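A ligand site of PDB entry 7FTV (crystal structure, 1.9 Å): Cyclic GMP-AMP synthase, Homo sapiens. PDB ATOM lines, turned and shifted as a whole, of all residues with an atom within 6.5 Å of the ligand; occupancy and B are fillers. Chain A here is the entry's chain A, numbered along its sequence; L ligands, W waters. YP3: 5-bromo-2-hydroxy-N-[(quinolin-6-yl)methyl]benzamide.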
ATOM      1  N   ALA A  87      -3.721  24.954  -6.613  1.00  0.00           N
ATOM      2  CA  ALA A  87      -5.063  24.837  -6.049  1.00  0.00           C
ATOM      3  C   ALA A  87      -5.094  24.286  -4.624  1.00  0.00           C
ATOM      4  O   ALA A  87      -6.151  24.327  -3.998  1.00  0.00           O
ATOM      5  CB  ALA A  87      -5.943  23.949  -6.924  1.00  0.00           C
ATOM      6  N   TYR A  88      -3.979  23.772  -4.105  1.00  0.00           N
ATOM      7  CA  TYR A  88      -3.952  23.147  -2.794  1.00  0.00           C
ATOM      8  C   TYR A  88      -3.065  23.940  -1.833  1.00  0.00           C
ATOM      9  O   TYR A  88      -2.021  24.463  -2.231  1.00  0.00           O
ATOM     10  CB  TYR A  88      -3.477  21.702  -2.886  1.00  0.00           C
ATOM     11  CG  TYR A  88      -4.493  20.797  -3.580  1.00  0.00           C
ATOM     12  CD1 TYR A  88      -4.569  20.713  -4.959  1.00  0.00           C
ATOM     13  CD2 TYR A  88      -5.353  19.993  -2.824  1.00  0.00           C
ATOM     14  CE1 TYR A  88      -5.498  19.866  -5.587  1.00  0.00           C
ATOM     15  CE2 TYR A  88      -6.281  19.137  -3.442  1.00  0.00           C
ATOM     16  CZ  TYR A  88      -6.349  19.084  -4.825  1.00  0.00           C
ATOM     17  OH  TYR A  88      -7.254  18.240  -5.426  1.00  0.00           O
ATOM     18  N   LYS A 202      -8.860  18.108   1.030  1.00  0.00           N
ATOM     19  CA  LYS A 202      -8.546  17.112  -0.010  1.00  0.00           C
ATOM     20  C   LYS A 202      -7.042  17.028  -0.198  1.00  0.00           C
ATOM     21  O   LYS A 202      -6.335  18.022   0.046  1.00  0.00           O
ATOM     22  CB  LYS A 202      -9.232  17.419  -1.363  1.00  0.00           C
ATOM     23  CG  LYS A 202      -9.152  16.261  -2.391  1.00  0.00           C
ATOM     24  CD  LYS A 202      -9.753  16.560  -3.795  1.00  0.00           C
ATOM     25  CE  LYS A 202      -9.484  15.374  -4.776  1.00  0.00           C
ATOM     26  NZ  LYS A 202     -10.224  15.410  -6.093  1.00  0.00           N
ATOM     27  N   ARG A 216      -8.401  22.639  -0.640  1.00  0.00           N
ATOM     28  CA  ARG A 216      -8.530  23.187  -1.983  1.00  0.00           C
ATOM     29  C   ARG A 216      -9.632  24.231  -2.022  1.00  0.00           C
ATOM     30  O   ARG A 216     -10.584  24.176  -1.253  1.00  0.00           O
ATOM     31  CB  ARG A 216      -8.803  22.108  -3.059  1.00  0.00           C
ATOM     32  CG  ARG A 216     -10.223  21.606  -3.178  1.00  0.00           C
ATOM     33  CD  ARG A 216     -10.416  20.975  -4.557  1.00  0.00           C
ATOM     34  NE  ARG A 216     -11.650  20.182  -4.672  1.00  0.00           N
ATOM     35  CZ  ARG A 216     -12.885  20.690  -4.668  1.00  0.00           C
ATOM     36  NH1 ARG A 216     -13.088  22.000  -4.554  1.00  0.00           N
ATOM     37  NH2 ARG A 216     -13.935  19.877  -4.777  1.00  0.00           N
ATOM     38  N   LEU A 217      -9.476  25.179  -2.934  1.00  0.00           N
ATOM     39  CA  LEU A 217     -10.482  26.208  -3.158  1.00  0.00           C
ATOM     40  C   LEU A 217     -11.781  25.609  -3.681  1.00  0.00           C
ATOM     41  O   LEU A 217     -11.770  24.660  -4.480  1.00  0.00           O
ATOM     42  CB  LEU A 217      -9.969  27.250  -4.154  1.00  0.00           C
ATOM     43  CG  LEU A 217      -8.856  28.149  -3.646  1.00  0.00           C
ATOM     44  CD1 LEU A 217      -8.010  28.678  -4.806  1.00  0.00           C
ATOM     45  CD2 LEU A 217      -9.520  29.281  -2.901  1.00  0.00           C
ATOM     46  N   SER A 218     -12.894  26.169  -3.222  1.00  0.00           N
ATOM     47  CA  SER A 218     -14.225  25.746  -3.621  1.00  0.00           C
ATOM     48  C   SER A 218     -15.026  26.973  -4.057  1.00  0.00           C
ATOM     49  O   SER A 218     -15.098  27.965  -3.312  1.00  0.00           O
ATOM     50  CB  SER A 218     -14.934  25.023  -2.477  1.00  0.00           C
ATOM     51  OG  SER A 218     -16.304  24.786  -2.740  1.00  0.00           O
ATOM     52  N   PHE A 219     -15.614  26.904  -5.257  1.00  0.00           N
ATOM     53  CA  PHE A 219     -16.284  28.047  -5.867  1.00  0.00           C
ATOM     54  C   PHE A 219     -17.730  27.739  -6.267  1.00  0.00           C
ATOM     55  O   PHE A 219     -18.268  28.370  -7.176  1.00  0.00           O
ATOM     56  CB  PHE A 219     -15.505  28.528  -7.096  1.00  0.00           C
ATOM     57  CG  PHE A 219     -14.172  29.118  -6.769  1.00  0.00           C
ATOM     58  CD1 PHE A 219     -14.092  30.387  -6.225  1.00  0.00           C
ATOM     59  CD2 PHE A 219     -12.997  28.420  -7.045  1.00  0.00           C
ATOM     60  CE1 PHE A 219     -12.875  30.958  -5.942  1.00  0.00           C
ATOM     61  CE2 PHE A 219     -11.749  29.004  -6.747  1.00  0.00           C
ATOM     62  CZ  PHE A 219     -11.688  30.262  -6.199  1.00  0.00           C
ATOM     63  N   SER A 220     -18.364  26.751  -5.612  1.00  0.00           N
ATOM     64  CA  SER A 220     -19.740  26.388  -5.958  1.00  0.00           C
ATOM     65  C   SER A 220     -20.696  27.579  -5.844  1.00  0.00           C
ATOM     66  O   SER A 220     -21.691  27.655  -6.584  1.00  0.00           O
ATOM     67  CB  SER A 220     -20.242  25.282  -5.039  1.00  0.00           C
ATOM     68  OG  SER A 220     -19.441  24.133  -5.165  1.00  0.00           O
ATOM     69  N   HIS A 221     -20.454  28.478  -4.904  1.00  0.00           N
ATOM     70  CA  HIS A 221     -21.311  29.637  -4.741  1.00  0.00           C
ATOM     71  C   HIS A 221     -21.180  30.610  -5.894  1.00  0.00           C
ATOM     72  O   HIS A 221     -22.168  31.260  -6.257  1.00  0.00           O
ATOM     73  CB  HIS A 221     -20.996  30.342  -3.414  1.00  0.00           C
ATOM     74  CG  HIS A 221     -19.593  30.850  -3.334  1.00  0.00           C
ATOM     75  ND1 HIS A 221     -18.487  30.068  -3.626  1.00  0.00           N
ATOM     76  CD2 HIS A 221     -19.105  32.068  -3.004  1.00  0.00           C
ATOM     77  CE1 HIS A 221     -17.395  30.786  -3.466  1.00  0.00           C
ATOM     78  NE2 HIS A 221     -17.739  32.004  -3.084  1.00  0.00           N
ATOM     79  N   GLU A 223     -20.334  29.592  -9.007  1.00  0.00           N
ATOM     80  CA  GLU A 223     -21.029  28.891 -10.091  1.00  0.00           C
ATOM     81  C   GLU A 223     -22.538  29.168 -10.025  1.00  0.00           C
ATOM     82  O   GLU A 223     -23.176  29.406 -11.056  1.00  0.00           O
ATOM     83  CB  GLU A 223     -20.780  27.385 -10.007  1.00  0.00           C
ATOM     84  CG  GLU A 223     -21.772  26.612 -10.854  1.00  0.00           C
ATOM     85  CD  GLU A 223     -21.745  25.113 -10.619  1.00  0.00           C
ATOM     86  OE1 GLU A 223     -21.133  24.660  -9.631  1.00  0.00           O
ATOM     87  OE2 GLU A 223     -22.352  24.382 -11.439  1.00  0.00           O
ATOM     88  N   SER A 274     -15.898  13.651 -13.036  1.00  0.00           N
ATOM     89  CA  SER A 274     -16.976  14.156 -12.195  1.00  0.00           C
ATOM     90  C   SER A 274     -17.596  15.379 -12.857  1.00  0.00           C
ATOM     91  O   SER A 274     -17.147  15.853 -13.909  1.00  0.00           O
ATOM     92  CB  SER A 274     -16.465  14.503 -10.800  1.00  0.00           C
ATOM     93  OG  SER A 274     -15.670  15.673 -10.893  1.00  0.00           O
ATOM     94  N   SER A 275     -18.644  15.902 -12.233  1.00  0.00           N
ATOM     95  CA  SER A 275     -19.327  17.080 -12.773  1.00  0.00           C
ATOM     96  C   SER A 275     -18.423  18.299 -12.792  1.00  0.00           C
ATOM     97  O   SER A 275     -18.709  19.254 -13.533  1.00  0.00           O
ATOM     98  CB  SER A 275     -20.581  17.383 -11.955  1.00  0.00           C
ATOM     99  OG  SER A 275     -20.208  17.818 -10.658  1.00  0.00           O
ATOM    100  N   TYR A 276     -17.352  18.311 -11.988  1.00  0.00           N
ATOM    101  CA  TYR A 276     -16.376  19.397 -12.110  1.00  0.00           C
ATOM    102  C   TYR A 276     -15.806  19.497 -13.508  1.00  0.00           C
ATOM    103  O   TYR A 276     -15.551  20.604 -14.019  1.00  0.00           O
ATOM    104  CB  TYR A 276     -15.229  19.193 -11.120  1.00  0.00           C
ATOM    105  CG  TYR A 276     -15.593  19.526  -9.706  1.00  0.00           C
ATOM    106  CD1 TYR A 276     -15.636  20.852  -9.301  1.00  0.00           C
ATOM    107  CD2 TYR A 276     -15.887  18.531  -8.783  1.00  0.00           C
ATOM    108  CE1 TYR A 276     -15.980  21.188  -8.032  1.00  0.00           C
ATOM    109  CE2 TYR A 276     -16.215  18.861  -7.475  1.00  0.00           C
ATOM    110  CZ  TYR A 276     -16.264  20.203  -7.111  1.00  0.00           C
ATOM    111  OH  TYR A 276     -16.599  20.590  -5.836  1.00  0.00           O
ATOM    112  N   HIS A 277     -15.498  18.364 -14.124  1.00  0.00           N
ATOM    113  CA  HIS A 277     -14.908  18.427 -15.462  1.00  0.00           C
ATOM    114  C   HIS A 277     -15.928  18.928 -16.468  1.00  0.00           C
ATOM    115  O   HIS A 277     -15.610  19.737 -17.343  1.00  0.00           O
ATOM    116  CB  HIS A 277     -14.352  17.051 -15.823  1.00  0.00           C
ATOM    117  CG  HIS A 277     -13.381  16.538 -14.809  1.00  0.00           C
ATOM    118  ND1 HIS A 277     -13.655  15.468 -13.994  1.00  0.00           N
ATOM    119  CD2 HIS A 277     -12.166  17.004 -14.427  1.00  0.00           C
ATOM    120  CE1 HIS A 277     -12.634  15.267 -13.179  1.00  0.00           C
ATOM    121  NE2 HIS A 277     -11.718  16.183 -13.424  1.00  0.00           N
ATOM    122  N   LYS A 279     -18.757  20.765 -15.809  1.00  0.00           N
ATOM    123  CA  LYS A 279     -19.077  22.167 -15.563  1.00  0.00           C
ATOM    124  C   LYS A 279     -17.978  23.066 -16.094  1.00  0.00           C
ATOM    125  O   LYS A 279     -18.261  24.099 -16.719  1.00  0.00           O
ATOM    126  CB  LYS A 279     -19.267  22.454 -14.069  1.00  0.00           C
ATOM    127  CG  LYS A 279     -20.418  21.771 -13.404  1.00  0.00           C
ATOM    128  CD  LYS A 279     -20.314  22.053 -11.909  1.00  0.00           C
ATOM    129  CE  LYS A 279     -21.393  21.362 -11.091  1.00  0.00           C
ATOM    130  NZ  LYS A 279     -21.090  21.542  -9.647  1.00  0.00           N
ATOM    131  N   THR A 280     -16.707  22.684 -15.868  1.00  0.00           N
ATOM    132  CA  THR A 280     -15.601  23.529 -16.295  1.00  0.00           C
ATOM    133  C   THR A 280     -15.564  23.684 -17.807  1.00  0.00           C
ATOM    134  O   THR A 280     -15.412  24.796 -18.324  1.00  0.00           O
ATOM    135  CB  THR A 280     -14.272  22.945 -15.790  1.00  0.00           C
ATOM    136  OG1 THR A 280     -14.306  22.915 -14.368  1.00  0.00           O
ATOM    137  CG2 THR A 280     -13.102  23.811 -16.258  1.00  0.00           C
ATOM    138  N   PHE A 283     -18.404  26.110 -18.933  1.00  0.00           N
ATOM    139  CA  PHE A 283     -18.166  27.544 -18.806  1.00  0.00           C
ATOM    140  C   PHE A 283     -17.109  28.024 -19.779  1.00  0.00           C
ATOM    141  O   PHE A 283     -17.147  29.191 -20.194  1.00  0.00           O
ATOM    142  CB  PHE A 283     -17.780  27.908 -17.365  1.00  0.00           C
ATOM    143  CG  PHE A 283     -18.929  27.843 -16.416  1.00  0.00           C
ATOM    144  CD1 PHE A 283     -20.098  28.549 -16.677  1.00  0.00           C
ATOM    145  CD2 PHE A 283     -18.867  27.059 -15.271  1.00  0.00           C
ATOM    146  CE1 PHE A 283     -21.157  28.474 -15.811  1.00  0.00           C
ATOM    147  CE2 PHE A 283     -19.925  26.985 -14.395  1.00  0.00           C
ATOM    148  CZ  PHE A 283     -21.083  27.682 -14.657  1.00  0.00           C
ATOM    149  N   ASN A 322      -8.656  24.687 -15.331  1.00  0.00           N
ATOM    150  CA  ASN A 322      -9.570  25.101 -14.283  1.00  0.00           C
ATOM    151  C   ASN A 322     -10.097  26.501 -14.575  1.00  0.00           C
ATOM    152  O   ASN A 322      -9.333  27.380 -14.988  1.00  0.00           O
ATOM    153  CB  ASN A 322      -8.848  25.075 -12.943  1.00  0.00           C
ATOM    154  CG  ASN A 322      -9.761  25.366 -11.786  1.00  0.00           C
ATOM    155  OD1 ASN A 322     -10.125  26.513 -11.569  1.00  0.00           O
ATOM    156  ND2 ASN A 322     -10.149  24.325 -11.049  1.00  0.00           N
ATOM    157  N   TYR A 323     -11.404  26.705 -14.391  1.00  0.00           N
ATOM    158  CA  TYR A 323     -12.021  27.963 -14.803  1.00  0.00           C
ATOM    159  C   TYR A 323     -11.640  29.109 -13.877  1.00  0.00           C
ATOM    160  O   TYR A 323     -11.716  30.276 -14.276  1.00  0.00           O
ATOM    161  CB  TYR A 323     -13.548  27.810 -14.859  1.00  0.00           C
ATOM    162  CG  TYR A 323     -14.275  28.858 -15.688  1.00  0.00           C
ATOM    163  CD1 TYR A 323     -14.137  28.895 -17.084  1.00  0.00           C
ATOM    164  CD2 TYR A 323     -15.102  29.813 -15.081  1.00  0.00           C
ATOM    165  CE1 TYR A 323     -14.789  29.850 -17.846  1.00  0.00           C
ATOM    166  CE2 TYR A 323     -15.765  30.788 -15.843  1.00  0.00           C
ATOM    167  CZ  TYR A 323     -15.611  30.787 -17.209  1.00  0.00           C
ATOM    168  OH  TYR A 323     -16.244  31.723 -17.982  1.00  0.00           O
ATOM    169  N   PHE A 324     -11.222  28.791 -12.639  1.00  0.00           N
ATOM    170  CA  PHE A 324     -10.866  29.790 -11.650  1.00  0.00           C
ATOM    171  C   PHE A 324      -9.365  29.900 -11.426  1.00  0.00           C
ATOM    172  O   PHE A 324      -8.902  30.954 -10.960  1.00  0.00           O
ATOM    173  CB  PHE A 324     -11.533  29.462 -10.294  1.00  0.00           C
ATOM    174  CG  PHE A 324     -13.027  29.594 -10.312  1.00  0.00           C
ATOM    175  CD1 PHE A 324     -13.828  28.545 -10.742  1.00  0.00           C
ATOM    176  CD2 PHE A 324     -13.622  30.790  -9.925  1.00  0.00           C
ATOM    177  CE1 PHE A 324     -15.223  28.682 -10.774  1.00  0.00           C
ATOM    178  CE2 PHE A 324     -14.998  30.926  -9.969  1.00  0.00           C
ATOM    179  CZ  PHE A 324     -15.789  29.888 -10.391  1.00  0.00           C
ATOM    180  N   ILE A 325      -8.611  28.860 -11.714  1.00  0.00           N
ATOM    181  CA  ILE A 325      -7.180  28.808 -11.470  1.00  0.00           C
ATOM    182  C   ILE A 325      -6.518  28.425 -12.789  1.00  0.00           C
ATOM    183  O   ILE A 325      -6.355  27.232 -13.088  1.00  0.00           O
ATOM    184  CB  ILE A 325      -6.850  27.806 -10.347  1.00  0.00           C
ATOM    185  CG1 ILE A 325      -7.773  28.060  -9.126  1.00  0.00           C
ATOM    186  CG2 ILE A 325      -5.383  27.895  -9.946  1.00  0.00           C
ATOM    187  CD1 ILE A 325      -7.935  26.851  -8.197  1.00  0.00           C
ATOM    188  N   PHE A 328      -3.941  25.402 -13.600  1.00  0.00           N
ATOM    189  CA  PHE A 328      -4.265  24.072 -13.076  1.00  0.00           C
ATOM    190  C   PHE A 328      -5.026  23.298 -14.146  1.00  0.00           C
ATOM    191  O   PHE A 328      -6.168  23.641 -14.478  1.00  0.00           O
ATOM    192  CB  PHE A 328      -5.083  24.204 -11.790  1.00  0.00           C
ATOM    193  CG  PHE A 328      -5.304  22.898 -11.099  1.00  0.00           C
ATOM    194  CD1 PHE A 328      -6.411  22.122 -11.384  1.00  0.00           C
ATOM    195  CD2 PHE A 328      -4.395  22.428 -10.160  1.00  0.00           C
ATOM    196  CE1 PHE A 328      -6.603  20.905 -10.753  1.00  0.00           C
ATOM    197  CE2 PHE A 328      -4.589  21.210  -9.539  1.00  0.00           C
ATOM    198  CZ  PHE A 328      -5.697  20.454  -9.825  1.00  0.00           C
ATOM    199  N   LEU A 330      -7.011  20.213 -15.082  1.00  0.00           N
ATOM    200  CA  LEU A 330      -7.809  19.119 -14.549  1.00  0.00           C
ATOM    201  C   LEU A 330      -7.548  17.807 -15.268  1.00  0.00           C
ATOM    202  O   LEU A 330      -7.795  16.744 -14.690  1.00  0.00           O
ATOM    203  CB  LEU A 330      -9.304  19.467 -14.652  1.00  0.00           C
ATOM    204  CG  LEU A 330      -9.755  20.618 -13.755  1.00  0.00           C
ATOM    205  CD1 LEU A 330     -11.146  20.956 -14.134  1.00  0.00           C
ATOM    206  CD2 LEU A 330      -9.704  20.205 -12.279  1.00  0.00           C
ATOM    207  N   LEU A 335      -3.163  13.482 -12.994  1.00  0.00           N
ATOM    208  CA  LEU A 335      -4.463  13.433 -12.329  1.00  0.00           C
ATOM    209  C   LEU A 335      -5.309  12.293 -12.889  1.00  0.00           C
ATOM    210  O   LEU A 335      -5.826  11.467 -12.138  1.00  0.00           O
ATOM    211  CB  LEU A 335      -5.185  14.772 -12.449  1.00  0.00           C
ATOM    212  CG  LEU A 335      -4.761  15.912 -11.509  1.00  0.00           C
ATOM    213  CD1 LEU A 335      -5.560  17.210 -11.758  1.00  0.00           C
ATOM    214  CD2 LEU A 335      -4.903  15.477 -10.046  1.00  0.00           C
HETATM  215  C10 YP3 L   1     -11.627  18.271  -8.606  1.00  0.00           C
HETATM  216  C11 YP3 L   1     -10.197  18.140  -8.681  1.00  0.00           C
HETATM  217  C13 YP3 L   1     -13.407  24.784  -9.039  1.00  0.00           C
HETATM  218  C15 YP3 L   1     -15.456  25.107 -10.451  1.00  0.00           C
HETATM  219  C16 YP3 L   1     -16.820  25.144 -10.510  1.00  0.00           C
HETATM  220  C17 YP3 L   1     -17.655  25.012  -9.428  1.00  0.00           C
HETATM  221  C18 YP3 L   1     -17.088  24.793  -8.176  1.00  0.00           C
HETATM  222  C19 YP3 L   1     -15.667  24.722  -8.081  1.00  0.00           C
HETATM  223  C14 YP3 L   1     -14.859  24.879  -9.202  1.00  0.00           C
HETATM  224  C2  YP3 L   1     -11.340  24.491  -7.632  1.00  0.00           C
HETATM  225  C3  YP3 L   1     -10.875  23.047  -7.865  1.00  0.00           C
HETATM  226  C4  YP3 L   1      -9.460  22.774  -7.948  1.00  0.00           C
HETATM  227  C5  YP3 L   1      -8.981  21.512  -8.174  1.00  0.00           C
HETATM  228  C6  YP3 L   1      -9.873  20.414  -8.326  1.00  0.00           C
HETATM  229  C7  YP3 L   1     -11.265  20.648  -8.233  1.00  0.00           C
HETATM  230  C8  YP3 L   1     -11.755  21.970  -7.999  1.00  0.00           C
HETATM  231  C9  YP3 L   1     -12.145  19.521  -8.374  1.00  0.00           C
HETATM  232  N1  YP3 L   1     -12.825  24.634  -7.804  1.00  0.00           N
HETATM  233  N12 YP3 L   1      -9.344  19.155  -8.549  1.00  0.00           N
HETATM  234  O20 YP3 L   1     -15.157  24.517  -6.873  1.00  0.00           O
HETATM  235  O22 YP3 L   1     -12.729  24.750 -10.059  1.00  0.00           O
HETATM  236 BR21 YP3 L   1     -17.561  25.497 -12.243  1.00  0.00          BR
HETATM  237  O   HOH W   1     -12.985  24.894 -12.886  1.00  0.00           O
HETATM  238  O   HOH W   2     -13.184  15.551  -9.331  1.00  0.00           O
HETATM  239  O   HOH W   3     -15.854  22.836  -5.143  1.00  0.00           O
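O of Leu 217 sits close to N1 of the ligand (3.5 Å). ND2 of Asn 322 lies within hydrogen-bond range of O22 of the ligand, at 2.8 Å. The backbone NH (N) of Phe 219 is in hydrogen-bond range of an oxygen (O20) of the ligand, at 2.9 Å.
N of Phe 324 is in hydrogen-bond range of OD1 of Asn 322 (2.7 Å). The backbone NH (N) of Asn 322 lies within hydrogen-bond range of the backbone carbonyl oxygen (O) of Phe 328 (2.8 Å). The backbone NH (N) of Tyr 276 lies close to the side-chain hydroxyl (OG) of Ser 274 (3.3 Å). OG1 of Thr 280 is in hydrogen-bond range of O of Tyr 276 (2.6 Å). The backbone carbonyl oxygen (O) of Phe 283 lies close to the side-chain hydroxyl (OH) of Tyr 323. The side-chain amide oxygen (OD1) of Asn 322 lies within hydrogen-bond range of the backbone NH (N) of Ile 325 (2.8 Å). OH of Tyr 276 lies within hydrogen-bond range of NH2 of Arg 216 (3.0 Å). The side-chain carboxylate (OE1) of Glu 223 is in salt-bridge range of the side-chain amino group (NZ) of Lys 279.
Residues that only touch the ligand: Ser 220 (3.5 Å), Glu 223 (3.5 Å), Phe 283 (3.5 Å), Tyr 276 (3.5 Å), Phe 328 (3.6 Å), Phe 324 (3.6 Å), Ser 218 (3.6 Å), Arg 216 (3.6 Å), Lys 202 (3.8 Å), Ala 87 (3.8 Å), Tyr 88 (3.9 Å), Leu 330 (3.9 Å) and Lys 279 (3.9 Å). Hydrophobic or aromatic side chains within 4 Å of the ligand: Ala 87, Phe 219, Tyr 276, Phe 283, Phe 324, Phe 328 and Leu 330. Within 4 Å of the ligand: Ala 87, Tyr 88, Lys 202, Arg 216, Leu 217, Ser 218, Phe 219, Ser 220, Glu 223, Tyr 276, Lys 279, Phe 283, Asn 322, Phe 324, Phe 328 and Leu 330.
Water W3 lies within hydrogen-bond range of the side-chain hydroxyl of Tyr 276 (2.5 Å), an oxygen (O20) of the ligand (2.5 Å), the guanidinium group of Arg 216 (2.9 Å) and the side-chain hydroxyl of Ser 218 (3.1 Å). Water W1 lies within hydrogen-bond range of the side-chain hydroxyl (OG1) of Thr 280 (2.8 Å), the backbone NH (N) of Tyr 323 (2.8 Å), an oxygen (O22) of the ligand (2.8 Å) and the side-chain amide nitrogen (ND2) of Asn 322 (3.4 Å).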
